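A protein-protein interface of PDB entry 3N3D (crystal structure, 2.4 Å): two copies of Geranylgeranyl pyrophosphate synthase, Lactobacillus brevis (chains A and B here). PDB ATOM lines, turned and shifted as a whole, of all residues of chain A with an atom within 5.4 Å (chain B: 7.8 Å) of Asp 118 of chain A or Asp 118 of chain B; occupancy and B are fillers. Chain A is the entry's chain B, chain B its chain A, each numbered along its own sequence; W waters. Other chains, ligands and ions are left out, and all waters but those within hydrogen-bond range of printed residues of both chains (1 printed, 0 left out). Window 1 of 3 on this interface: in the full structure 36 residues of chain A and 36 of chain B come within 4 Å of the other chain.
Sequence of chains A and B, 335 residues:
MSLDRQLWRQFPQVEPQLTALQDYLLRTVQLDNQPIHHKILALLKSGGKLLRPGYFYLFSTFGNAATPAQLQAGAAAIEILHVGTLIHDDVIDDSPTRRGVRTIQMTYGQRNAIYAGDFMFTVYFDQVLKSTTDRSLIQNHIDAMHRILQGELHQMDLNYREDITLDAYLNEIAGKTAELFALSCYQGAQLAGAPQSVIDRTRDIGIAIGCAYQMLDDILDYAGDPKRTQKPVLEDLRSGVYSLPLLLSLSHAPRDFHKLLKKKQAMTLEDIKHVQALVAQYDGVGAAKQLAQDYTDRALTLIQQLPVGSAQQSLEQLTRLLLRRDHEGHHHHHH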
ATOM      1  N   HIS A  88       3.751  27.723  17.142  1.00  0.00           N
ATOM      2  CA  HIS A  88       4.220  26.720  16.195  1.00  0.00           C
ATOM      3  C   HIS A  88       5.459  27.151  15.413  1.00  0.00           C
ATOM      4  O   HIS A  88       6.181  26.309  14.873  1.00  0.00           O
ATOM      5  CB  HIS A  88       3.084  26.292  15.265  1.00  0.00           C
ATOM      6  CG  HIS A  88       2.151  25.296  15.884  1.00  0.00           C
ATOM      7  ND1 HIS A  88       1.126  24.698  15.185  1.00  0.00           N
ATOM      8  CD2 HIS A  88       2.100  24.781  17.138  1.00  0.00           C
ATOM      9  CE1 HIS A  88       0.476  23.869  15.984  1.00  0.00           C
ATOM     10  NE2 HIS A  88       1.054  23.892  17.171  1.00  0.00           N
ATOM     11  N   ALA A 113       4.410  22.740  23.190  1.00  0.00           N
ATOM     12  CA  ALA A 113       4.265  23.795  22.196  1.00  0.00           C
ATOM     13  C   ALA A 113       3.318  23.386  21.061  1.00  0.00           C
ATOM     14  O   ALA A 113       2.404  24.136  20.720  1.00  0.00           O
ATOM     15  CB  ALA A 113       5.627  24.205  21.650  1.00  0.00           C
ATOM     16  N   ILE A 114       3.525  22.196  20.501  1.00  0.00           N
ATOM     17  CA  ILE A 114       2.636  21.653  19.475  1.00  0.00           C
ATOM     18  C   ILE A 114       1.174  21.605  19.938  1.00  0.00           C
ATOM     19  O   ILE A 114       0.282  22.114  19.244  1.00  0.00           O
ATOM     20  CB  ILE A 114       3.060  20.251  19.063  1.00  0.00           C
ATOM     21  CG1 ILE A 114       4.501  20.273  18.575  1.00  0.00           C
ATOM     22  CG2 ILE A 114       2.127  19.711  17.985  1.00  0.00           C
ATOM     23  CD1 ILE A 114       5.158  18.928  18.598  1.00  0.00           C
ATOM     24  N   TYR A 115       0.950  21.015  21.115  1.00  0.00           N
ATOM     25  CA  TYR A 115      -0.381  20.930  21.718  1.00  0.00           C
ATOM     26  C   TYR A 115      -0.982  22.289  22.039  1.00  0.00           C
ATOM     27  O   TYR A 115      -2.180  22.474  21.859  1.00  0.00           O
ATOM     28  CB  TYR A 115      -0.379  20.060  22.986  1.00  0.00           C
ATOM     29  CG  TYR A 115      -0.176  18.579  22.733  1.00  0.00           C
ATOM     30  CD1 TYR A 115       0.556  17.795  23.630  1.00  0.00           C
ATOM     31  CD2 TYR A 115      -0.699  17.964  21.594  1.00  0.00           C
ATOM     32  CE1 TYR A 115       0.750  16.432  23.406  1.00  0.00           C
ATOM     33  CE2 TYR A 115      -0.503  16.611  21.355  1.00  0.00           C
ATOM     34  CZ  TYR A 115       0.217  15.847  22.266  1.00  0.00           C
ATOM     35  OH  TYR A 115       0.412  14.502  22.034  1.00  0.00           O
ATOM     36  N   ALA A 116      -0.154  23.225  22.510  1.00  0.00           N
ATOM     37  CA  ALA A 116      -0.612  24.582  22.830  1.00  0.00           C
ATOM     38  C   ALA A 116      -1.137  25.307  21.598  1.00  0.00           C
ATOM     39  O   ALA A 116      -2.144  25.993  21.684  1.00  0.00           O
ATOM     40  CB  ALA A 116       0.496  25.410  23.491  1.00  0.00           C
ATOM     41  N   GLY A 117      -0.449  25.131  20.468  1.00  0.00           N
ATOM     42  CA  GLY A 117      -0.815  25.761  19.211  1.00  0.00           C
ATOM     43  C   GLY A 117      -2.090  25.165  18.661  1.00  0.00           C
ATOM     44  O   GLY A 117      -2.957  25.896  18.160  1.00  0.00           O
ATOM     45  N   ASP A 118      -2.200  23.838  18.777  1.00  0.00           N
ATOM     46  CA  ASP A 118      -3.385  23.089  18.345  1.00  0.00           C
ATOM     47  C   ASP A 118      -4.615  23.435  19.162  1.00  0.00           C
ATOM     48  O   ASP A 118      -5.712  23.552  18.619  1.00  0.00           O
ATOM     49  CB  ASP A 118      -3.112  21.596  18.399  1.00  0.00           C
ATOM     50  CG  ASP A 118      -2.215  21.141  17.273  1.00  0.00           C
ATOM     51  OD1 ASP A 118      -1.920  21.964  16.378  1.00  0.00           O
ATOM     52  OD2 ASP A 118      -1.804  19.965  17.278  1.00  0.00           O
ATOM     53  N   PHE A 119      -4.408  23.610  20.464  1.00  0.00           N
ATOM     54  CA  PHE A 119      -5.425  24.134  21.361  1.00  0.00           C
ATOM     55  C   PHE A 119      -5.885  25.517  20.902  1.00  0.00           C
ATOM     56  O   PHE A 119      -7.080  25.781  20.846  1.00  0.00           O
ATOM     57  CB  PHE A 119      -4.880  24.219  22.792  1.00  0.00           C
ATOM     58  CG  PHE A 119      -5.814  24.877  23.766  1.00  0.00           C
ATOM     59  CD1 PHE A 119      -7.024  24.279  24.112  1.00  0.00           C
ATOM     60  CD2 PHE A 119      -5.471  26.087  24.360  1.00  0.00           C
ATOM     61  CE1 PHE A 119      -7.891  24.891  25.025  1.00  0.00           C
ATOM     62  CE2 PHE A 119      -6.321  26.708  25.272  1.00  0.00           C
ATOM     63  CZ  PHE A 119      -7.535  26.106  25.611  1.00  0.00           C
ATOM     64  N   MET A 120      -4.926  26.384  20.579  1.00  0.00           N
ATOM     65  CA  MET A 120      -5.236  27.729  20.111  1.00  0.00           C
ATOM     66  C   MET A 120      -6.073  27.702  18.818  1.00  0.00           C
ATOM     67  O   MET A 120      -7.047  28.438  18.717  1.00  0.00           O
ATOM     68  CB  MET A 120      -3.968  28.581  19.985  1.00  0.00           C
ATOM     69  CG  MET A 120      -3.324  28.935  21.343  1.00  0.00           C
ATOM     70  SD  MET A 120      -4.463  29.724  22.497  1.00  0.00           S
ATOM     71  CE  MET A 120      -4.087  31.429  22.128  1.00  0.00           C
ATOM     72  N   PHE A 121      -5.756  26.799  17.889  1.00  0.00           N
ATOM     73  CA  PHE A 121      -6.558  26.641  16.675  1.00  0.00           C
ATOM     74  C   PHE A 121      -8.002  26.202  16.920  1.00  0.00           C
ATOM     75  O   PHE A 121      -8.892  26.617  16.182  1.00  0.00           O
ATOM     76  CB  PHE A 121      -5.878  25.714  15.660  1.00  0.00           C
ATOM     77  CG  PHE A 121      -4.550  26.219  15.171  1.00  0.00           C
ATOM     78  CD1 PHE A 121      -4.324  27.591  14.990  1.00  0.00           C
ATOM     79  CD2 PHE A 121      -3.525  25.328  14.872  1.00  0.00           C
ATOM     80  CE1 PHE A 121      -3.083  28.064  14.543  1.00  0.00           C
ATOM     81  CE2 PHE A 121      -2.282  25.794  14.417  1.00  0.00           C
ATOM     82  CZ  PHE A 121      -2.063  27.161  14.252  1.00  0.00           C
ATOM     83  N   THR A 122      -8.243  25.384  17.943  1.00  0.00           N
ATOM     84  CA  THR A 122      -9.610  24.964  18.260  1.00  0.00           C
ATOM     85  C   THR A 122     -10.389  26.112  18.889  1.00  0.00           C
ATOM     86  O   THR A 122     -11.584  26.282  18.625  1.00  0.00           O
ATOM     87  CB  THR A 122      -9.678  23.700  19.181  1.00  0.00           C
ATOM     88  OG1 THR A 122      -9.126  23.999  20.466  1.00  0.00           O
ATOM     89  CG2 THR A 122      -8.917  22.528  18.577  1.00  0.00           C
ATOM     90  N   VAL A 123      -9.705  26.898  19.717  1.00  0.00           N
ATOM     91  CA  VAL A 123     -10.306  28.076  20.359  1.00  0.00           C
ATOM     92  C   VAL A 123     -10.569  29.184  19.321  1.00  0.00           C
ATOM     93  O   VAL A 123     -11.581  29.895  19.394  1.00  0.00           O
ATOM     94  CB  VAL A 123      -9.416  28.596  21.524  1.00  0.00           C
ATOM     95  CG1 VAL A 123      -9.959  29.896  22.107  1.00  0.00           C
ATOM     96  CG2 VAL A 123      -9.308  27.547  22.631  1.00  0.00           C
ATOM     97  N   LEU A 149      -0.764  29.557   6.448  1.00  0.00           N
ATOM     98  CA  LEU A 149      -0.101  28.263   6.553  1.00  0.00           C
ATOM     99  C   LEU A 149       0.463  27.759   5.230  1.00  0.00           C
ATOM    100  O   LEU A 149       1.354  26.911   5.220  1.00  0.00           O
ATOM    101  CB  LEU A 149      -1.013  27.240   7.230  1.00  0.00           C
ATOM    102  CG  LEU A 149      -1.242  27.592   8.707  1.00  0.00           C
ATOM    103  CD1 LEU A 149      -2.428  26.864   9.257  1.00  0.00           C
ATOM    104  CD2 LEU A 149      -0.008  27.318   9.565  1.00  0.00           C
ATOM    105  N   GLY B  84      -4.752  14.765   9.762  1.00  0.00           N
ATOM    106  CA  GLY B  84      -4.080  15.892  10.394  1.00  0.00           C
ATOM    107  C   GLY B  84      -3.615  15.633  11.815  1.00  0.00           C
ATOM    108  O   GLY B  84      -2.520  16.054  12.192  1.00  0.00           O
ATOM    109  N   THR B  85      -4.445  14.952  12.609  1.00  0.00           N
ATOM    110  CA  THR B  85      -4.067  14.603  13.983  1.00  0.00           C
ATOM    111  C   THR B  85      -2.973  13.540  13.959  1.00  0.00           C
ATOM    112  O   THR B  85      -2.046  13.603  14.753  1.00  0.00           O
ATOM    113  CB  THR B  85      -5.266  14.139  14.869  1.00  0.00           C
ATOM    114  OG1 THR B  85      -6.033  13.153  14.177  1.00  0.00           O
ATOM    115  CG2 THR B  85      -6.177  15.301  15.220  1.00  0.00           C
ATOM    116  N   ILE B  87      -0.588  13.124  11.682  1.00  0.00           N
ATOM    117  CA  ILE B  87       0.649  13.820  11.330  1.00  0.00           C
ATOM    118  C   ILE B  87       1.295  14.417  12.585  1.00  0.00           C
ATOM    119  O   ILE B  87       2.493  14.255  12.808  1.00  0.00           O
ATOM    120  CB  ILE B  87       0.388  14.912  10.245  1.00  0.00           C
ATOM    121  CG1 ILE B  87       0.184  14.270   8.869  1.00  0.00           C
ATOM    122  CG2 ILE B  87       1.523  15.915  10.178  1.00  0.00           C
ATOM    123  CD1 ILE B  87      -0.433  15.207   7.816  1.00  0.00           C
ATOM    124  N   HIS B  88       0.486  15.067  13.411  1.00  0.00           N
ATOM    125  CA  HIS B  88       0.943  15.615  14.680  1.00  0.00           C
ATOM    126  C   HIS B  88       1.310  14.568  15.730  1.00  0.00           C
ATOM    127  O   HIS B  88       2.295  14.739  16.445  1.00  0.00           O
ATOM    128  CB  HIS B  88      -0.097  16.588  15.242  1.00  0.00           C
ATOM    129  CG  HIS B  88      -0.023  17.947  14.625  1.00  0.00           C
ATOM    130  ND1 HIS B  88      -0.632  19.051  15.177  1.00  0.00           N
ATOM    131  CD2 HIS B  88       0.612  18.382  13.509  1.00  0.00           C
ATOM    132  CE1 HIS B  88      -0.392  20.105  14.417  1.00  0.00           C
ATOM    133  NE2 HIS B  88       0.364  19.728  13.402  1.00  0.00           N
ATOM    134  N   ASP B  89       0.520  13.496  15.817  1.00  0.00           N
ATOM    135  CA  ASP B  89       0.789  12.403  16.756  1.00  0.00           C
ATOM    136  C   ASP B  89       2.099  11.705  16.435  1.00  0.00           C
ATOM    137  O   ASP B  89       2.808  11.274  17.339  1.00  0.00           O
ATOM    138  CB  ASP B  89      -0.355  11.385  16.772  1.00  0.00           C
ATOM    139  CG  ASP B  89      -1.621  11.935  17.412  1.00  0.00           C
ATOM    140  OD1 ASP B  89      -1.530  12.890  18.217  1.00  0.00           O
ATOM    141  OD2 ASP B  89      -2.715  11.414  17.105  1.00  0.00           O
ATOM    142  N   ILE B  92       4.962  13.920  17.901  1.00  0.00           N
ATOM    143  CA  ILE B  92       5.054  13.713  19.352  1.00  0.00           C
ATOM    144  C   ILE B  92       5.641  12.349  19.741  1.00  0.00           C
ATOM    145  O   ILE B  92       6.548  12.278  20.571  1.00  0.00           O
ATOM    146  CB  ILE B  92       3.683  13.970  20.049  1.00  0.00           C
ATOM    147  CG1 ILE B  92       3.511  15.459  20.330  1.00  0.00           C
ATOM    148  CG2 ILE B  92       3.545  13.217  21.374  1.00  0.00           C
ATOM    149  CD1 ILE B  92       2.623  16.166  19.354  1.00  0.00           C
ATOM    150  N   ARG B 111       9.149  20.774  11.921  1.00  0.00           N
ATOM    151  CA  ARG B 111       8.341  21.987  11.815  1.00  0.00           C
ATOM    152  C   ARG B 111       7.432  21.938  10.601  1.00  0.00           C
ATOM    153  O   ARG B 111       6.262  22.307  10.679  1.00  0.00           O
ATOM    154  CB  ARG B 111       9.207  23.247  11.786  1.00  0.00           C
ATOM    155  CG  ARG B 111       8.410  24.501  12.101  1.00  0.00           C
ATOM    156  CD  ARG B 111       9.255  25.545  12.768  1.00  0.00           C
ATOM    157  NE  ARG B 111       9.616  26.649  11.887  1.00  0.00           N
ATOM    158  CZ  ARG B 111      10.494  27.597  12.202  1.00  0.00           C
ATOM    159  NH1 ARG B 111      10.751  28.572  11.342  1.00  0.00           N
ATOM    160  NH2 ARG B 111      11.123  27.570  13.372  1.00  0.00           N
ATOM    161  N   ASN B 112       7.981  21.450   9.496  1.00  0.00           N
ATOM    162  CA  ASN B 112       7.230  21.250   8.271  1.00  0.00           C
ATOM    163  C   ASN B 112       6.090  20.241   8.435  1.00  0.00           C
ATOM    164  O   ASN B 112       5.006  20.424   7.873  1.00  0.00           O
ATOM    165  CB  ASN B 112       8.178  20.844   7.148  1.00  0.00           C
ATOM    166  CG  ASN B 112       9.223  21.915   6.850  1.00  0.00           C
ATOM    167  OD1 ASN B 112       9.029  23.100   7.139  1.00  0.00           O
ATOM    168  ND2 ASN B 112      10.340  21.496   6.273  1.00  0.00           N
ATOM    169  N   ALA B 113       6.338  19.195   9.223  1.00  0.00           N
ATOM    170  CA  ALA B 113       5.308  18.236   9.598  1.00  0.00           C
ATOM    171  C   ALA B 113       4.217  18.890  10.444  1.00  0.00           C
ATOM    172  O   ALA B 113       3.040  18.585  10.288  1.00  0.00           O
ATOM    173  CB  ALA B 113       5.916  17.072  10.342  1.00  0.00           C
ATOM    174  N   ILE B 114       4.605  19.793  11.335  1.00  0.00           N
ATOM    175  CA  ILE B 114       3.625  20.485  12.158  1.00  0.00           C
ATOM    176  C   ILE B 114       2.776  21.399  11.284  1.00  0.00           C
ATOM    177  O   ILE B 114       1.548  21.371  11.383  1.00  0.00           O
ATOM    178  CB  ILE B 114       4.289  21.219  13.345  1.00  0.00           C
ATOM    179  CG1 ILE B 114       4.605  20.203  14.443  1.00  0.00           C
ATOM    180  CG2 ILE B 114       3.388  22.326  13.918  1.00  0.00           C
ATOM    181  CD1 ILE B 114       5.868  20.500  15.190  1.00  0.00           C
ATOM    182  N   TYR B 115       3.441  22.149  10.402  1.00  0.00           N
ATOM    183  CA  TYR B 115       2.775  23.036   9.450  1.00  0.00           C
ATOM    184  C   TYR B 115       1.815  22.284   8.533  1.00  0.00           C
ATOM    185  O   TYR B 115       0.705  22.759   8.290  1.00  0.00           O
ATOM    186  CB  TYR B 115       3.787  23.827   8.607  1.00  0.00           C
ATOM    187  CG  TYR B 115       4.535  24.919   9.342  1.00  0.00           C
ATOM    188  CD1 TYR B 115       5.824  25.292   8.943  1.00  0.00           C
ATOM    189  CD2 TYR B 115       3.964  25.580  10.437  1.00  0.00           C
ATOM    190  CE1 TYR B 115       6.523  26.293   9.614  1.00  0.00           C
ATOM    191  CE2 TYR B 115       4.656  26.581  11.122  1.00  0.00           C
ATOM    192  CZ  TYR B 115       5.935  26.926  10.708  1.00  0.00           C
ATOM    193  OH  TYR B 115       6.616  27.918  11.371  1.00  0.00           O
ATOM    194  N   ALA B 116       2.242  21.115   8.047  1.00  0.00           N
ATOM    195  CA  ALA B 116       1.384  20.244   7.241  1.00  0.00           C
ATOM    196  C   ALA B 116       0.144  19.790   8.018  1.00  0.00           C
ATOM    197  O   ALA B 116      -0.960  19.768   7.468  1.00  0.00           O
ATOM    198  CB  ALA B 116       2.155  19.052   6.720  1.00  0.00           C
ATOM    199  N   GLY B 117       0.328  19.457   9.293  1.00  0.00           N
ATOM    200  CA  GLY B 117      -0.790  19.113  10.166  1.00  0.00           C
ATOM    201  C   GLY B 117      -1.732  20.290  10.333  1.00  0.00           C
ATOM    202  O   GLY B 117      -2.950  20.134  10.234  1.00  0.00           O
ATOM    203  N   ASP B 118      -1.160  21.468  10.570  1.00  0.00           N
ATOM    204  CA  ASP B 118      -1.915  22.724  10.693  1.00  0.00           C
ATOM    205  C   ASP B 118      -2.720  23.046   9.429  1.00  0.00           C
ATOM    206  O   ASP B 118      -3.875  23.464   9.509  1.00  0.00           O
ATOM    207  CB  ASP B 118      -0.958  23.887  10.987  1.00  0.00           C
ATOM    208  CG  ASP B 118      -0.317  23.794  12.360  1.00  0.00           C
ATOM    209  OD1 ASP B 118      -0.819  23.033  13.214  1.00  0.00           O
ATOM    210  OD2 ASP B 118       0.695  24.496  12.586  1.00  0.00           O
ATOM    211  N   PHE B 119      -2.083  22.836   8.279  1.00  0.00           N
ATOM    212  CA  PHE B 119      -2.695  22.987   6.976  1.00  0.00           C
ATOM    213  C   PHE B 119      -3.938  22.115   6.829  1.00  0.00           C
ATOM    214  O   PHE B 119      -4.972  22.586   6.350  1.00  0.00           O
ATOM    215  CB  PHE B 119      -1.675  22.652   5.879  1.00  0.00           C
ATOM    216  CG  PHE B 119      -2.253  22.617   4.490  1.00  0.00           C
ATOM    217  CD1 PHE B 119      -2.605  23.797   3.834  1.00  0.00           C
ATOM    218  CD2 PHE B 119      -2.424  21.407   3.825  1.00  0.00           C
ATOM    219  CE1 PHE B 119      -3.138  23.768   2.547  1.00  0.00           C
ATOM    220  CE2 PHE B 119      -2.960  21.369   2.532  1.00  0.00           C
ATOM    221  CZ  PHE B 119      -3.318  22.548   1.895  1.00  0.00           C
ATOM    222  N   MET B 120      -3.831  20.854   7.239  1.00  0.00           N
ATOM    223  CA  MET B 120      -4.954  19.931   7.189  1.00  0.00           C
ATOM    224  C   MET B 120      -6.141  20.419   8.035  1.00  0.00           C
ATOM    225  O   MET B 120      -7.288  20.281   7.620  1.00  0.00           O
ATOM    226  CB  MET B 120      -4.521  18.516   7.593  1.00  0.00           C
ATOM    227  CG  MET B 120      -3.526  17.879   6.620  1.00  0.00           C
ATOM    228  SD  MET B 120      -4.224  17.671   4.979  1.00  0.00           S
ATOM    229  CE  MET B 120      -4.994  16.084   5.193  1.00  0.00           C
ATOM    230  N   PHE B 121      -5.866  21.039   9.179  1.00  0.00           N
ATOM    231  CA  PHE B 121      -6.927  21.650   9.984  1.00  0.00           C
ATOM    232  C   PHE B 121      -7.680  22.755   9.235  1.00  0.00           C
ATOM    233  O   PHE B 121      -8.882  22.931   9.448  1.00  0.00           O
ATOM    234  CB  PHE B 121      -6.410  22.170  11.344  1.00  0.00           C
ATOM    235  CG  PHE B 121      -5.762  21.109  12.206  1.00  0.00           C
ATOM    236  CD1 PHE B 121      -6.202  19.783  12.176  1.00  0.00           C
ATOM    237  CD2 PHE B 121      -4.723  21.443  13.065  1.00  0.00           C
ATOM    238  CE1 PHE B 121      -5.593  18.809  12.966  1.00  0.00           C
ATOM    239  CE2 PHE B 121      -4.118  20.473  13.863  1.00  0.00           C
ATOM    240  CZ  PHE B 121      -4.555  19.157  13.809  1.00  0.00           C
ATOM    241  N   THR B 122      -6.986  23.478   8.357  1.00  0.00           N
ATOM    242  CA  THR B 122      -7.647  24.510   7.546  1.00  0.00           C
ATOM    243  C   THR B 122      -8.523  23.888   6.468  1.00  0.00           C
ATOM    244  O   THR B 122      -9.620  24.368   6.215  1.00  0.00           O
ATOM    245  CB  THR B 122      -6.656  25.518   6.916  1.00  0.00           C
ATOM    246  OG1 THR B 122      -6.018  24.944   5.765  1.00  0.00           O
ATOM    247  CG2 THR B 122      -5.608  25.904   7.921  1.00  0.00           C
ATOM    248  N   VAL B 123      -8.039  22.815   5.850  1.00  0.00           N
ATOM    249  CA  VAL B 123      -8.842  22.040   4.908  1.00  0.00           C
ATOM    250  C   VAL B 123     -10.044  21.390   5.620  1.00  0.00           C
ATOM    251  O   VAL B 123     -11.153  21.346   5.071  1.00  0.00           O
ATOM    252  CB  VAL B 123      -7.986  20.979   4.164  1.00  0.00           C
ATOM    253  CG1 VAL B 123      -8.816  20.229   3.155  1.00  0.00           C
ATOM    254  CG2 VAL B 123      -6.834  21.647   3.438  1.00  0.00           C
ATOM    255  N   TYR B 124      -9.818  20.917   6.847  1.00  0.00           N
ATOM    256  CA  TYR B 124     -10.867  20.311   7.666  1.00  0.00           C
ATOM    257  C   TYR B 124     -12.032  21.260   7.886  1.00  0.00           C
ATOM    258  O   TYR B 124     -13.171  20.914   7.591  1.00  0.00           O
ATOM    259  CB  TYR B 124     -10.285  19.838   9.008  1.00  0.00           C
ATOM    260  CG  TYR B 124     -11.297  19.583  10.104  1.00  0.00           C
ATOM    261  CD1 TYR B 124     -11.287  20.350  11.272  1.00  0.00           C
ATOM    262  CD2 TYR B 124     -12.260  18.580   9.980  1.00  0.00           C
ATOM    263  CE1 TYR B 124     -12.202  20.121  12.292  1.00  0.00           C
ATOM    264  CE2 TYR B 124     -13.186  18.345  10.993  1.00  0.00           C
ATOM    265  CZ  TYR B 124     -13.145  19.119  12.150  1.00  0.00           C
ATOM    266  OH  TYR B 124     -14.052  18.904  13.155  1.00  0.00           O
ATOM    267  N   MET B 145     -13.093  18.299  18.274  1.00  0.00           N
ATOM    268  CA  MET B 145     -11.671  18.626  18.091  1.00  0.00           C
ATOM    269  C   MET B 145     -11.029  18.951  19.440  1.00  0.00           C
ATOM    270  O   MET B 145      -9.920  18.498  19.733  1.00  0.00           O
ATOM    271  CB  MET B 145     -11.499  19.803  17.117  1.00  0.00           C
ATOM    272  CG  MET B 145     -10.253  19.730  16.195  1.00  0.00           C
ATOM    273  SD  MET B 145      -9.902  21.264  15.266  1.00  0.00           S
ATOM    274  CE  MET B 145     -11.520  22.025  15.396  1.00  0.00           C
ATOM    275  N   HIS B 146     -11.752  19.708  20.264  1.00  0.00           N
ATOM    276  CA  HIS B 146     -11.355  20.001  21.640  1.00  0.00           C
ATOM    277  C   HIS B 146     -11.232  18.729  22.495  1.00  0.00           C
ATOM    278  O   HIS B 146     -10.304  18.612  23.295  1.00  0.00           O
ATOM    279  CB  HIS B 146     -12.350  20.986  22.267  1.00  0.00           C
ATOM    280  CG  HIS B 146     -11.953  21.474  23.625  1.00  0.00           C
ATOM    281  ND1 HIS B 146     -10.864  22.292  23.834  1.00  0.00           N
ATOM    282  CD2 HIS B 146     -12.510  21.270  24.844  1.00  0.00           C
ATOM    283  CE1 HIS B 146     -10.758  22.559  25.124  1.00  0.00           C
ATOM    284  NE2 HIS B 146     -11.747  21.955  25.759  1.00  0.00           N
ATOM    285  N   LEU B 149      -8.044  16.582  21.495  1.00  0.00           N
ATOM    286  CA  LEU B 149      -6.856  17.192  22.075  1.00  0.00           C
ATOM    287  C   LEU B 149      -6.766  16.961  23.591  1.00  0.00           C
ATOM    288  O   LEU B 149      -5.685  16.694  24.110  1.00  0.00           O
ATOM    289  CB  LEU B 149      -6.821  18.687  21.757  1.00  0.00           C
ATOM    290  CG  LEU B 149      -5.747  19.514  22.460  1.00  0.00           C
ATOM    291  CD1 LEU B 149      -4.529  19.688  21.575  1.00  0.00           C
ATOM    292  CD2 LEU B 149      -6.330  20.841  22.876  1.00  0.00           C
ATOM    293  N   GLU B 152      -5.433  13.766  24.155  1.00  0.00           N
ATOM    294  CA  GLU B 152      -4.024  13.698  23.813  1.00  0.00           C
ATOM    295  C   GLU B 152      -3.178  14.132  25.011  1.00  0.00           C
ATOM    296  O   GLU B 152      -2.116  13.559  25.266  1.00  0.00           O
ATOM    297  CB  GLU B 152      -3.745  14.569  22.587  1.00  0.00           C
ATOM    298  CG  GLU B 152      -2.779  13.956  21.601  1.00  0.00           C
ATOM    299  CD  GLU B 152      -3.332  12.744  20.901  1.00  0.00           C
ATOM    300  OE1 GLU B 152      -2.926  11.622  21.273  1.00  0.00           O
ATOM    301  OE2 GLU B 152      -4.164  12.912  19.983  1.00  0.00           O
HETATM  302  O   HOH W   1      -0.635  12.089  23.505  1.00  0.00           O
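ND1 of His 88 of chain B is in hydrogen-bond range of OD2 of Asp 118 of chain A, 2.6 Å away. ND1 of His 88 of chain A is in hydrogen-bond range of OD2 of Asp 118 of chain B (2.6 Å).
A ring nitrogen (NE2) of His 88 of chain B lies within hydrogen-bond range of the backbone carbonyl oxygen (O) of Ile 114 of chain B (2.9 Å). A ring nitrogen (NE2) of His 88 of chain A sits at hydrogen-bond distance from the backbone carbonyl oxygen (O) of Ile 114 of chain A (2.8 Å). The backbone carbonyl oxygen of Phe 119 of chain A lies within hydrogen-bond range of the side-chain hydroxyl of Thr 122 of chain A (2.7 Å).
Arg 111 of chain B touches His 88 of chain A. His 88 of chain B touches Ile 114 of chain A. CD1 of Ile 114 of chain A touches CD1 of Ile 92 of chain B, at 3.8 Å. O of Tyr 115 of chain A touches CD1 of Leu 149 of chain B, 3.7 Å away. OH of Tyr 115 of chain A touches CG of Glu 152 of chain B (3.3 Å). Asp 118 of chain A touches Asp 118 of chain B. CE1 of His 146 of chain B touches CE1 of Phe 119 of chain A, 3.7 Å away. Phe 121 of chain A touches Asp 118 of chain B. CG2 of Thr 122 of chain A touches SD of Met 145 of chain B, 3.7 Å away.
Printed residues of chain B within 4 Å of His 88 of chain A: Arg 111 (3.8 Å), Ile 114 (3.5 Å), Tyr 115 (3.9 Å) and Asp 118 (2.6 Å). No residue of chain B comes within 4 Å of Gly 117 of chain A. Asp 118 of chain A touches four residues of chain B. Gly 84 of chain B touches none of the printed residues of chain A. Of the printed residues of chain A, Tyr 115 of chain B touches His 88. The nearest printed residue of chain B that does not touch Asp 118 of chain A is Met 145 of chain B (5.8 Å).
Of the 13 printed residues of chain A, 8 touch a printed residue of chain B. Hydrophobic or aromatic side chains of chain A that line the printed part of chain B: His 88, Ile 114, Tyr 115, Phe 119, Phe 121 and Leu 149. Hydrophobic or aromatic side chains of chain B that line the printed part of chain A: His 88, Ile 92, Ile 114, Tyr 115, Phe 121, Met 145, His 146 and Leu 149. Among the printed residues, 20 pairs touch across the chains. Among the printed residues, no Asp or Glu carboxylate lies within 4 Å of a Lys or Arg side-chain nitrogen of the other chain.
His 88 of chain A touches Tyr 115 of chain B, but with the chains exchanged Tyr 115 of chain A does not touch His 88 of chain B (5.9 Å). Ile 114 of chain A touches its own counterpart, Ile 114 of chain B. Asp 118 of chain A touches its own counterpart, Asp 118 of chain B. Leu 149 of chain A touches Thr 122 of chain B, but with the chains exchanged Thr 122 of chain A does not touch Leu 149 of chain B (4.9 Å). Positions printed for both chains: 88, 113, 114, 115, 116, 117, 118, 119, 120, 121, 122, 123 and 149.
Water W1 lies within hydrogen-bond range of O of Glu 152 of chain B (2.7 Å) and OH of Tyr 115 of chain A (3.0 Å).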
